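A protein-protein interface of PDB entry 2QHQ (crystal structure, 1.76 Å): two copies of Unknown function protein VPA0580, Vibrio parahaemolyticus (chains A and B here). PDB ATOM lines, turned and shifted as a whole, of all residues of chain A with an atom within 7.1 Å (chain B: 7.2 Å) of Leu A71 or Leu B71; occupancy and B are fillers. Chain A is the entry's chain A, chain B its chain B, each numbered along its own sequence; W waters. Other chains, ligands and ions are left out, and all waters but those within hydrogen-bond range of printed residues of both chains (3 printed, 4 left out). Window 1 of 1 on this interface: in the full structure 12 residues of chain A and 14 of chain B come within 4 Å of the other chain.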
ATOM      1  N   MLY A  65      -8.459  20.385  16.802  1.00  0.00           N
ATOM      2  CA  MLY A  65      -7.889  19.218  16.128  1.00  0.00           C
ATOM      3  CB  MLY A  65      -8.556  17.934  16.624  1.00  0.00           C
ATOM      4  CG  MLY A  65      -8.067  17.569  18.016  1.00  0.00           C
ATOM      5  CD  MLY A  65      -8.775  16.275  18.411  1.00  0.00           C
ATOM      6  CE  MLY A  65      -8.154  15.593  19.628  1.00  0.00           C
ATOM      7  NZ  MLY A  65      -8.949  14.381  19.739  1.00  0.00           N
ATOM      8  CH1 MLY A  65      -8.488  13.144  19.108  1.00  0.00           C
ATOM      9  CH2 MLY A  65     -10.238  14.437  20.427  1.00  0.00           C
ATOM     10  C   MLY A  65      -8.060  19.278  14.631  1.00  0.00           C
ATOM     11  O   MLY A  65      -7.132  18.994  13.882  1.00  0.00           O
ATOM     12  N   ILE A  66      -9.255  19.635  14.171  1.00  0.00           N
ATOM     13  CA  ILE A  66      -9.491  19.617  12.726  1.00  0.00           C
ATOM     14  C   ILE A  66      -8.630  20.654  11.998  1.00  0.00           C
ATOM     15  O   ILE A  66      -8.046  20.349  10.950  1.00  0.00           O
ATOM     16  CB  ILE A  66     -10.994  19.725  12.355  1.00  0.00           C
ATOM     17  CG1 ILE A  66     -11.686  18.402  12.738  1.00  0.00           C
ATOM     18  CG2 ILE A  66     -11.141  20.071  10.843  1.00  0.00           C
ATOM     19  CD1 ILE A  66     -13.249  18.404  12.675  1.00  0.00           C
ATOM     20  N   PHE A  67      -8.560  21.881  12.531  1.00  0.00           N
ATOM     21  CA  PHE A  67      -7.737  22.896  11.885  1.00  0.00           C
ATOM     22  C   PHE A  67      -6.269  22.511  11.905  1.00  0.00           C
ATOM     23  O   PHE A  67      -5.582  22.681  10.904  1.00  0.00           O
ATOM     24  CB  PHE A  67      -7.963  24.301  12.479  1.00  0.00           C
ATOM     25  CG  PHE A  67      -9.361  24.814  12.259  1.00  0.00           C
ATOM     26  CD1 PHE A  67      -9.956  24.732  11.002  1.00  0.00           C
ATOM     27  CD2 PHE A  67     -10.082  25.377  13.308  1.00  0.00           C
ATOM     28  CE1 PHE A  67     -11.250  25.205  10.797  1.00  0.00           C
ATOM     29  CE2 PHE A  67     -11.380  25.839  13.102  1.00  0.00           C
ATOM     30  CZ  PHE A  67     -11.956  25.745  11.851  1.00  0.00           C
ATOM     31  N   ALA A  68      -5.785  21.984  13.027  1.00  0.00           N
ATOM     32  CA  ALA A  68      -4.388  21.526  13.091  1.00  0.00           C
ATOM     33  C   ALA A  68      -4.128  20.413  12.082  1.00  0.00           C
ATOM     34  O   ALA A  68      -3.098  20.394  11.425  1.00  0.00           O
ATOM     35  CB  ALA A  68      -4.014  21.069  14.519  1.00  0.00           C
ATOM     36  N   PHE A  69      -5.078  19.488  11.966  1.00  0.00           N
ATOM     37  CA  PHE A  69      -4.988  18.365  11.036  1.00  0.00           C
ATOM     38  C   PHE A  69      -4.974  18.877   9.585  1.00  0.00           C
ATOM     39  O   PHE A  69      -4.213  18.402   8.760  1.00  0.00           O
ATOM     40  CB  PHE A  69      -6.204  17.452  11.273  1.00  0.00           C
ATOM     41  CG  PHE A  69      -6.309  16.314  10.305  1.00  0.00           C
ATOM     42  CD1 PHE A  69      -5.558  15.154  10.502  1.00  0.00           C
ATOM     43  CD2 PHE A  69      -7.159  16.402   9.189  1.00  0.00           C
ATOM     44  CE1 PHE A  69      -5.654  14.082   9.622  1.00  0.00           C
ATOM     45  CE2 PHE A  69      -7.240  15.341   8.278  1.00  0.00           C
ATOM     46  CZ  PHE A  69      -6.490  14.168   8.506  1.00  0.00           C
ATOM     47  N   GLY A  70      -5.836  19.852   9.283  1.00  0.00           N
ATOM     48  CA  GLY A  70      -5.839  20.458   7.945  1.00  0.00           C
ATOM     49  C   GLY A  70      -4.483  21.051   7.593  1.00  0.00           C
ATOM     50  O   GLY A  70      -4.021  20.938   6.456  1.00  0.00           O
ATOM     51  N   LEU A  71      -3.831  21.681   8.561  1.00  0.00           N
ATOM     52  CA  LEU A  71      -2.575  22.359   8.257  1.00  0.00           C
ATOM     53  C   LEU A  71      -1.472  21.329   8.045  1.00  0.00           C
ATOM     54  O   LEU A  71      -0.646  21.452   7.143  1.00  0.00           O
ATOM     55  CB  LEU A  71      -2.203  23.327   9.368  1.00  0.00           C
ATOM     56  CG  LEU A  71      -3.123  24.541   9.417  1.00  0.00           C
ATOM     57  CD1 LEU A  71      -2.848  25.368  10.650  1.00  0.00           C
ATOM     58  CD2 LEU A  71      -2.981  25.333   8.119  1.00  0.00           C
ATOM     59  N   LEU A  72      -1.459  20.310   8.890  1.00  0.00           N
ATOM     60  CA  LEU A  72      -0.428  19.281   8.791  1.00  0.00           C
ATOM     61  C   LEU A  72      -0.533  18.481   7.487  1.00  0.00           C
ATOM     62  O   LEU A  72       0.460  17.929   7.015  1.00  0.00           O
ATOM     63  CB  LEU A  72      -0.473  18.336   9.999  1.00  0.00           C
ATOM     64  CG  LEU A  72      -0.037  18.888  11.360  1.00  0.00           C
ATOM     65  CD1 LEU A  72      -0.029  17.757  12.400  1.00  0.00           C
ATOM     66  CD2 LEU A  72       1.351  19.523  11.263  1.00  0.00           C
ATOM     67  N   ASN A  73      -1.732  18.422   6.915  1.00  0.00           N
ATOM     68  CA  ASN A  73      -1.968  17.633   5.699  1.00  0.00           C
ATOM     69  C   ASN A  73      -2.295  18.469   4.459  1.00  0.00           C
ATOM     70  O   ASN A  73      -2.785  17.950   3.455  1.00  0.00           O
ATOM     71  CB  ASN A  73      -3.028  16.568   5.980  1.00  0.00           C
ATOM     72  CG  ASN A  73      -2.540  15.555   6.987  1.00  0.00           C
ATOM     73  OD1 ASN A  73      -1.670  14.742   6.676  1.00  0.00           O
ATOM     74  ND2 ASN A  73      -3.027  15.644   8.213  1.00  0.00           N
ATOM     75  N   ALA A  74      -1.959  19.758   4.540  1.00  0.00           N
ATOM     76  CA  ALA A  74      -2.042  20.691   3.410  1.00  0.00           C
ATOM     77  C   ALA A  74      -3.441  20.782   2.788  1.00  0.00           C
ATOM     78  O   ALA A  74      -3.576  20.865   1.553  1.00  0.00           O
ATOM     79  CB  ALA A  74      -1.002  20.323   2.337  1.00  0.00           C
ATOM     80  N   LEU A  75      -4.474  20.727   3.628  1.00  0.00           N
ATOM     81  CA  LEU A  75      -5.849  20.775   3.125  1.00  0.00           C
ATOM     82  C   LEU A  75      -6.285  22.201   2.871  1.00  0.00           C
ATOM     83  O   LEU A  75      -5.943  23.096   3.634  1.00  0.00           O
ATOM     84  CB  LEU A  75      -6.815  20.140   4.136  1.00  0.00           C
ATOM     85  CG  LEU A  75      -6.577  18.666   4.461  1.00  0.00           C
ATOM     86  CD1 LEU A  75      -7.692  18.179   5.387  1.00  0.00           C
ATOM     87  CD2 LEU A  75      -6.501  17.801   3.184  1.00  0.00           C
ATOM     88  N   THR A  80     -11.030  21.089   4.466  1.00  0.00           N
ATOM     89  CA  THR A  80     -11.043  21.206   5.922  1.00  0.00           C
ATOM     90  C   THR A  80     -12.478  21.270   6.470  1.00  0.00           C
ATOM     91  O   THR A  80     -12.833  20.558   7.423  1.00  0.00           O
ATOM     92  CB  THR A  80     -10.177  22.405   6.385  1.00  0.00           C
ATOM     93  OG1 THR A  80      -8.844  22.243   5.875  1.00  0.00           O
ATOM     94  CG2 THR A  80     -10.100  22.486   7.912  1.00  0.00           C
ATOM     95  N   TRP A 112      -8.016  30.194   6.117  1.00  0.00           N
ATOM     96  CA  TRP A 112      -6.722  30.012   6.774  1.00  0.00           C
ATOM     97  C   TRP A 112      -6.108  31.351   7.139  1.00  0.00           C
ATOM     98  O   TRP A 112      -5.338  31.429   8.083  1.00  0.00           O
ATOM     99  CB  TRP A 112      -5.769  29.213   5.897  1.00  0.00           C
ATOM    100  CG  TRP A 112      -6.103  27.755   5.775  1.00  0.00           C
ATOM    101  CD1 TRP A 112      -6.317  27.066   4.623  1.00  0.00           C
ATOM    102  CD2 TRP A 112      -6.245  26.803   6.848  1.00  0.00           C
ATOM    103  NE1 TRP A 112      -6.594  25.741   4.905  1.00  0.00           N
ATOM    104  CE2 TRP A 112      -6.551  25.553   6.258  1.00  0.00           C
ATOM    105  CE3 TRP A 112      -6.153  26.889   8.250  1.00  0.00           C
ATOM    106  CZ2 TRP A 112      -6.740  24.382   7.017  1.00  0.00           C
ATOM    107  CZ3 TRP A 112      -6.348  25.732   9.006  1.00  0.00           C
ATOM    108  CH2 TRP A 112      -6.646  24.490   8.385  1.00  0.00           C
ATOM    109  N   ILE A 115      -6.754  32.095  10.716  1.00  0.00           N
ATOM    110  CA  ILE A 115      -6.326  31.075  11.705  1.00  0.00           C
ATOM    111  C   ILE A 115      -4.906  31.384  12.182  1.00  0.00           C
ATOM    112  O   ILE A 115      -4.016  31.612  11.364  1.00  0.00           O
ATOM    113  CB  ILE A 115      -6.369  29.628  11.076  1.00  0.00           C
ATOM    114  CG1 ILE A 115      -7.814  29.136  10.903  1.00  0.00           C
ATOM    115  CG2 ILE A 115      -5.582  28.607  11.899  1.00  0.00           C
ATOM    116  CD1 ILE A 115      -8.524  28.743  12.196  1.00  0.00           C
ATOM    117  N   GLN A 116      -4.711  31.370  13.507  1.00  0.00           N
ATOM    118  CA  GLN A 116      -3.409  31.549  14.116  1.00  0.00           C
ATOM    119  C   GLN A 116      -3.350  30.690  15.387  1.00  0.00           C
ATOM    120  O   GLN A 116      -4.101  30.946  16.323  1.00  0.00           O
ATOM    121  CB  GLN A 116      -3.247  33.046  14.424  1.00  0.00           C
ATOM    122  CG  GLN A 116      -2.098  33.480  15.300  1.00  0.00           C
ATOM    123  CD  GLN A 116      -2.034  34.995  15.403  1.00  0.00           C
ATOM    124  OE1 GLN A 116      -1.626  35.672  14.460  1.00  0.00           O
ATOM    125  NE2 GLN A 116      -2.434  35.538  16.550  1.00  0.00           N
ATOM    126  N   PHE A 117      -2.478  29.683  15.402  1.00  0.00           N
ATOM    127  CA  PHE A 117      -2.259  28.850  16.599  1.00  0.00           C
ATOM    128  C   PHE A 117      -1.134  29.429  17.432  1.00  0.00           C
ATOM    129  O   PHE A 117      -0.116  29.848  16.882  1.00  0.00           O
ATOM    130  CB  PHE A 117      -1.871  27.414  16.208  1.00  0.00           C
ATOM    131  CG  PHE A 117      -3.039  26.562  15.829  1.00  0.00           C
ATOM    132  CD1 PHE A 117      -3.711  25.808  16.793  1.00  0.00           C
ATOM    133  CD2 PHE A 117      -3.483  26.516  14.507  1.00  0.00           C
ATOM    134  CE1 PHE A 117      -4.811  25.025  16.455  1.00  0.00           C
ATOM    135  CE2 PHE A 117      -4.587  25.749  14.162  1.00  0.00           C
ATOM    136  CZ  PHE A 117      -5.255  24.997  15.143  1.00  0.00           C
ATOM    137  N   SER A 120       1.487  24.238  18.740  1.00  0.00           N
ATOM    138  CA  SER A 120       1.140  23.159  17.827  1.00  0.00           C
ATOM    139  C   SER A 120       0.263  22.114  18.544  1.00  0.00           C
ATOM    140  O   SER A 120       0.653  21.581  19.590  1.00  0.00           O
ATOM    141  CB  SER A 120       2.432  22.542  17.303  1.00  0.00           C
ATOM    142  OG  SER A 120       2.170  21.705  16.206  1.00  0.00           O
ATOM    143  N   MLY B  65      12.539  27.209  11.729  1.00  0.00           N
ATOM    144  CA  MLY B  65      11.717  28.283  12.297  1.00  0.00           C
ATOM    145  CB  MLY B  65      12.615  29.464  12.667  1.00  0.00           C
ATOM    146  CG  MLY B  65      13.385  29.216  13.953  1.00  0.00           C
ATOM    147  CD  MLY B  65      14.319  30.421  14.213  1.00  0.00           C
ATOM    148  CE  MLY B  65      15.177  30.056  15.418  1.00  0.00           C
ATOM    149  NZ  MLY B  65      16.185  31.061  15.724  1.00  0.00           N
ATOM    150  CH1 MLY B  65      16.953  30.873  16.959  1.00  0.00           C
ATOM    151  CH2 MLY B  65      16.436  32.218  14.878  1.00  0.00           C
ATOM    152  C   MLY B  65      10.649  28.770  11.345  1.00  0.00           C
ATOM    153  O   MLY B  65       9.485  28.965  11.730  1.00  0.00           O
ATOM    154  N   ILE B  66      11.029  28.976  10.091  1.00  0.00           N
ATOM    155  CA  ILE B  66      10.080  29.520   9.114  1.00  0.00           C
ATOM    156  C   ILE B  66       8.940  28.529   8.833  1.00  0.00           C
ATOM    157  O   ILE B  66       7.763  28.919   8.814  1.00  0.00           O
ATOM    158  CB  ILE B  66      10.785  30.026   7.839  1.00  0.00           C
ATOM    159  CG1 ILE B  66      11.591  31.297   8.176  1.00  0.00           C
ATOM    160  CG2 ILE B  66       9.751  30.351   6.739  1.00  0.00           C
ATOM    161  CD1 ILE B  66      12.321  31.931   6.968  1.00  0.00           C
ATOM    162  N   PHE B  67       9.273  27.249   8.622  1.00  0.00           N
ATOM    163  CA  PHE B  67       8.201  26.272   8.411  1.00  0.00           C
ATOM    164  C   PHE B  67       7.319  26.083   9.643  1.00  0.00           C
ATOM    165  O   PHE B  67       6.099  25.919   9.502  1.00  0.00           O
ATOM    166  CB  PHE B  67       8.738  24.941   7.890  1.00  0.00           C
ATOM    167  CG  PHE B  67       9.353  25.060   6.548  1.00  0.00           C
ATOM    168  CD1 PHE B  67       8.567  25.441   5.461  1.00  0.00           C
ATOM    169  CD2 PHE B  67      10.710  24.797   6.353  1.00  0.00           C
ATOM    170  CE1 PHE B  67       9.120  25.579   4.193  1.00  0.00           C
ATOM    171  CE2 PHE B  67      11.286  24.939   5.059  1.00  0.00           C
ATOM    172  CZ  PHE B  67      10.493  25.331   4.000  1.00  0.00           C
ATOM    173  N   ALA B  68       7.916  26.107  10.839  1.00  0.00           N
ATOM    174  CA  ALA B  68       7.101  25.995  12.050  1.00  0.00           C
ATOM    175  C   ALA B  68       6.136  27.199  12.161  1.00  0.00           C
ATOM    176  O   ALA B  68       4.962  27.043  12.514  1.00  0.00           O
ATOM    177  CB  ALA B  68       7.990  25.883  13.277  1.00  0.00           C
ATOM    178  N   PHE B  69       6.647  28.372  11.807  1.00  0.00           N
ATOM    179  CA  PHE B  69       5.886  29.625  11.801  1.00  0.00           C
ATOM    180  C   PHE B  69       4.761  29.553  10.767  1.00  0.00           C
ATOM    181  O   PHE B  69       3.627  29.987  11.034  1.00  0.00           O
ATOM    182  CB  PHE B  69       6.869  30.780  11.538  1.00  0.00           C
ATOM    183  CG  PHE B  69       6.219  32.130  11.384  1.00  0.00           C
ATOM    184  CD1 PHE B  69       5.875  32.870  12.509  1.00  0.00           C
ATOM    185  CD2 PHE B  69       5.975  32.661  10.120  1.00  0.00           C
ATOM    186  CE1 PHE B  69       5.290  34.143  12.379  1.00  0.00           C
ATOM    187  CE2 PHE B  69       5.393  33.950   9.965  1.00  0.00           C
ATOM    188  CZ  PHE B  69       5.061  34.686  11.106  1.00  0.00           C
ATOM    189  N   GLY B  70       5.074  28.998   9.592  1.00  0.00           N
ATOM    190  CA  GLY B  70       4.076  28.838   8.524  1.00  0.00           C
ATOM    191  C   GLY B  70       2.956  27.908   8.946  1.00  0.00           C
ATOM    192  O   GLY B  70       1.776  28.126   8.597  1.00  0.00           O
ATOM    193  N   LEU B  71       3.306  26.864   9.709  1.00  0.00           N
ATOM    194  CA  LEU B  71       2.288  25.959  10.229  1.00  0.00           C
ATOM    195  C   LEU B  71       1.408  26.615  11.290  1.00  0.00           C
ATOM    196  O   LEU B  71       0.182  26.497  11.220  1.00  0.00           O
ATOM    197  CB  LEU B  71       2.895  24.666  10.778  1.00  0.00           C
ATOM    198  CG  LEU B  71       3.309  23.643   9.728  1.00  0.00           C
ATOM    199  CD1 LEU B  71       4.055  22.504  10.426  1.00  0.00           C
ATOM    200  CD2 LEU B  71       2.050  23.140   8.964  1.00  0.00           C
ATOM    201  N   LEU B  72       2.012  27.291  12.267  1.00  0.00           N
ATOM    202  CA  LEU B  72       1.212  27.920  13.325  1.00  0.00           C
ATOM    203  C   LEU B  72       0.258  28.973  12.759  1.00  0.00           C
ATOM    204  O   LEU B  72      -0.855  29.116  13.241  1.00  0.00           O
ATOM    205  CB  LEU B  72       2.099  28.519  14.417  1.00  0.00           C
ATOM    206  CG  LEU B  72       2.868  27.524  15.318  1.00  0.00           C
ATOM    207  CD1 LEU B  72       3.665  28.312  16.367  1.00  0.00           C
ATOM    208  CD2 LEU B  72       1.894  26.586  16.002  1.00  0.00           C
ATOM    209  N   ASN B  73       0.698  29.685  11.725  1.00  0.00           N
ATOM    210  CA  ASN B  73      -0.080  30.801  11.165  1.00  0.00           C
ATOM    211  C   ASN B  73      -0.838  30.471   9.875  1.00  0.00           C
ATOM    212  O   ASN B  73      -1.387  31.359   9.223  1.00  0.00           O
ATOM    213  CB  ASN B  73       0.830  32.005  10.984  1.00  0.00           C
ATOM    214  CG  ASN B  73       1.267  32.559  12.311  1.00  0.00           C
ATOM    215  OD1 ASN B  73       0.435  33.008  13.086  1.00  0.00           O
ATOM    216  ND2 ASN B  73       2.539  32.456  12.612  1.00  0.00           N
ATOM    217  N   ALA B  74      -0.869  29.188   9.532  1.00  0.00           N
ATOM    218  CA  ALA B  74      -1.661  28.680   8.411  1.00  0.00           C
ATOM    219  C   ALA B  74      -1.311  29.362   7.089  1.00  0.00           C
ATOM    220  O   ALA B  74      -2.181  29.664   6.277  1.00  0.00           O
ATOM    221  CB  ALA B  74      -3.180  28.770   8.729  1.00  0.00           C
ATOM    222  N   LEU B  75      -0.014  29.573   6.873  1.00  0.00           N
ATOM    223  CA  LEU B  75       0.457  30.287   5.681  1.00  0.00           C
ATOM    224  C   LEU B  75       0.454  29.361   4.480  1.00  0.00           C
ATOM    225  O   LEU B  75       0.833  28.210   4.609  1.00  0.00           O
ATOM    226  CB  LEU B  75       1.874  30.830   5.921  1.00  0.00           C
ATOM    227  CG  LEU B  75       2.031  31.862   7.050  1.00  0.00           C
ATOM    228  CD1 LEU B  75       3.496  32.319   7.117  1.00  0.00           C
ATOM    229  CD2 LEU B  75       1.130  33.056   6.809  1.00  0.00           C
ATOM    230  N   THR B  80       4.698  31.266   2.613  1.00  0.00           N
ATOM    231  CA  THR B  80       5.808  30.661   3.368  1.00  0.00           C
ATOM    232  C   THR B  80       7.130  30.888   2.631  1.00  0.00           C
ATOM    233  O   THR B  80       8.124  31.317   3.225  1.00  0.00           O
ATOM    234  CB  THR B  80       5.535  29.168   3.601  1.00  0.00           C
ATOM    235  OG1 THR B  80       4.267  29.031   4.272  1.00  0.00           O
ATOM    236  CG2 THR B  80       6.647  28.544   4.469  1.00  0.00           C
ATOM    237  N   TRP B 112       3.703  21.932   1.232  1.00  0.00           N
ATOM    238  CA  TRP B 112       3.346  21.514   2.593  1.00  0.00           C
ATOM    239  C   TRP B 112       3.106  20.020   2.709  1.00  0.00           C
ATOM    240  O   TRP B 112       3.297  19.442   3.790  1.00  0.00           O
ATOM    241  CB  TRP B 112       2.115  22.267   3.089  1.00  0.00           C
ATOM    242  CG  TRP B 112       2.415  23.673   3.557  1.00  0.00           C
ATOM    243  CD1 TRP B 112       1.894  24.836   3.037  1.00  0.00           C
ATOM    244  CD2 TRP B 112       3.253  24.064   4.657  1.00  0.00           C
ATOM    245  NE1 TRP B 112       2.384  25.931   3.729  1.00  0.00           N
ATOM    246  CE2 TRP B 112       3.204  25.486   4.737  1.00  0.00           C
ATOM    247  CE3 TRP B 112       4.048  23.358   5.579  1.00  0.00           C
ATOM    248  CZ2 TRP B 112       3.916  26.215   5.707  1.00  0.00           C
ATOM    249  CZ3 TRP B 112       4.750  24.069   6.533  1.00  0.00           C
ATOM    250  CH2 TRP B 112       4.687  25.494   6.595  1.00  0.00           C
ATOM    251  N   GLU B 113       2.693  19.401   1.604  1.00  0.00           N
ATOM    252  CA  GLU B 113       2.518  17.956   1.542  1.00  0.00           C
ATOM    253  C   GLU B 113       3.808  17.227   1.914  1.00  0.00           C
ATOM    254  O   GLU B 113       3.781  16.175   2.528  1.00  0.00           O
ATOM    255  CB  GLU B 113       2.090  17.554   0.135  1.00  0.00           C
ATOM    256  CG  GLU B 113       0.683  17.984  -0.220  1.00  0.00           C
ATOM    257  CD  GLU B 113       0.575  19.329  -0.928  1.00  0.00           C
ATOM    258  OE1 GLU B 113       1.488  20.186  -0.826  1.00  0.00           O
ATOM    259  OE2 GLU B 113      -0.459  19.516  -1.604  1.00  0.00           O
ATOM    260  N   ILE B 115       6.191  18.331   3.917  1.00  0.00           N
ATOM    261  CA  ILE B 115       6.757  18.721   5.218  1.00  0.00           C
ATOM    262  C   ILE B 115       6.255  17.766   6.294  1.00  0.00           C
ATOM    263  O   ILE B 115       5.075  17.459   6.324  1.00  0.00           O
ATOM    264  CB  ILE B 115       6.352  20.173   5.598  1.00  0.00           C
ATOM    265  CG1 ILE B 115       7.107  21.207   4.725  1.00  0.00           C
ATOM    266  CG2 ILE B 115       6.540  20.424   7.125  1.00  0.00           C
ATOM    267  CD1 ILE B 115       8.616  21.312   5.010  1.00  0.00           C
ATOM    268  N   GLN B 116       7.143  17.301   7.172  1.00  0.00           N
ATOM    269  CA  GLN B 116       6.735  16.515   8.338  1.00  0.00           C
ATOM    270  C   GLN B 116       7.702  16.819   9.470  1.00  0.00           C
ATOM    271  O   GLN B 116       8.895  16.526   9.356  1.00  0.00           O
ATOM    272  CB  GLN B 116       6.757  15.019   8.016  1.00  0.00           C
ATOM    273  CG  GLN B 116       6.483  14.096   9.209  1.00  0.00           C
ATOM    274  CD  GLN B 116       5.148  13.386   9.138  1.00  0.00           C
ATOM    275  OE1 GLN B 116       4.321  13.643   8.256  1.00  0.00           O
ATOM    276  NE2 GLN B 116       4.943  12.453  10.057  1.00  0.00           N
ATOM    277  N   PHE B 117       7.190  17.439  10.528  1.00  0.00           N
ATOM    278  CA  PHE B 117       7.973  17.674  11.754  1.00  0.00           C
ATOM    279  C   PHE B 117       7.905  16.471  12.676  1.00  0.00           C
ATOM    280  O   PHE B 117       6.844  15.834  12.816  1.00  0.00           O
ATOM    281  CB  PHE B 117       7.430  18.890  12.501  1.00  0.00           C
ATOM    282  CG  PHE B 117       7.943  20.200  11.991  1.00  0.00           C
ATOM    283  CD1 PHE B 117       9.044  20.800  12.591  1.00  0.00           C
ATOM    284  CD2 PHE B 117       7.303  20.861  10.939  1.00  0.00           C
ATOM    285  CE1 PHE B 117       9.528  22.025  12.156  1.00  0.00           C
ATOM    286  CE2 PHE B 117       7.794  22.088  10.478  1.00  0.00           C
ATOM    287  CZ  PHE B 117       8.913  22.672  11.101  1.00  0.00           C
HETATM  288  O   HOH W   1       0.807  32.242  15.975  1.00  0.00           O
HETATM  289  O   HOH W   2      -2.019  21.668  -0.809  1.00  0.00           O
HETATM  290  O   HOH W   3       2.609  16.088   8.908  1.00  0.00           O
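The backbone carbonyl oxygen of Leu B72 is in hydrogen-bond range of the backbone NH of Phe A117 (2.8 Å).
The backbone carbonyl oxygen (O) of Asn B73 sits close to the backbone carbonyl oxygen (O) of Ile A115, 3.4 Å away.
NE1 of Trp A112 lies within hydrogen-bond range of O of Leu A75, at 3.0 Å.
O of Phe B69 sits at hydrogen-bond distance from ND2 of Asn B73.
The backbone carbonyl oxygen (O) of Leu B75 is in hydrogen-bond range of the indole nitrogen (NE1) of Trp B112, 2.9 Å away.
Among the printed residues, pairs that only touch across the chains: Leu A71 with Leu B71 (3.3 Å), Leu A71 with Ala B74 (3.5 Å), Ala A74 with Trp B112 (3.7 Å), Ala A74 with Glu B113 (3.8 Å), Trp A112 with Ala B74 (3.5 Å), Ile A115 with Ala B74 (3.96 Å), Gln A116 with Leu B72 (3.6 Å), Gln A116 with Asn B73 (3.4 Å) and Ser A120 with Leu B72 (3.6 Å).
Of the printed residues of chain B, Leu A71 touches Leu B71 and Ala B74.
Of chain A, only Leu A71 comes within 4 Å of Leu B71.
Gly B70 touches none of the printed residues of chain A.
Of the printed residues of chain B, Ile A115 touches Asn B73 and Ala B74.
Of the printed residues of chain B, Ala A74 touches Trp B112 (3.7 Å) and Glu B113 (3.8 Å).
Phe A69 touches none of the printed residues of chain B.
Gln B116 touches none of the printed residues of chain A.
The nearest residue of chain A that does not touch Leu B71 is Leu A72 (4.1 Å).
The nearest printed residue of chain B that does not touch Ala A74 is Leu B71 (6.9 Å).
Printed residues of chain A that touch a printed residue of chain B: Leu A71, Ala A74, Trp A112, Ile A115, Gln A116, Phe A117 and Ser A120.
Printed residues of chain B that touch a printed residue of chain A: Leu B71, Leu B72, Asn B73, Ala B74, Trp B112 and Glu B113.
Hydrophobic or aromatic side chains of chain B within 4 Å of the printed part of chain A: Leu B71, Leu B72, Ala B74 and Trp B112.
Among the printed residues, 11 pairs touch across the chains.
Among the printed residues, no Asp or Glu carboxylate lies within 4 Å of a Lys or Arg side-chain nitrogen of the other chain.
Ala A74 touches Trp B112, and with the chains exchanged Trp A112 touches Ala B74.
Ile A115 touches Ala B74, but with the chains exchanged Ala A74 does not touch Ile B115 (7.6 Å).
Gln A116 touches Leu B72, but with the chains exchanged Leu A72 does not touch Gln B116 (5.9 Å).
Gln A116 touches Asn B73, but with the chains exchanged Asn A73 does not touch Gln B116 (6.3 Å).
Water W1 bridges O of Phe A117 and OD1 of Asn B73.
Water W2 bridges OE2 of Glu B113 (2.8 Å) and O of Ala A74 (2.9 Å).
Water W3 bridges OE1 of Gln B116 (3.1 Å) and O of Leu A72 (3.4 Å).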
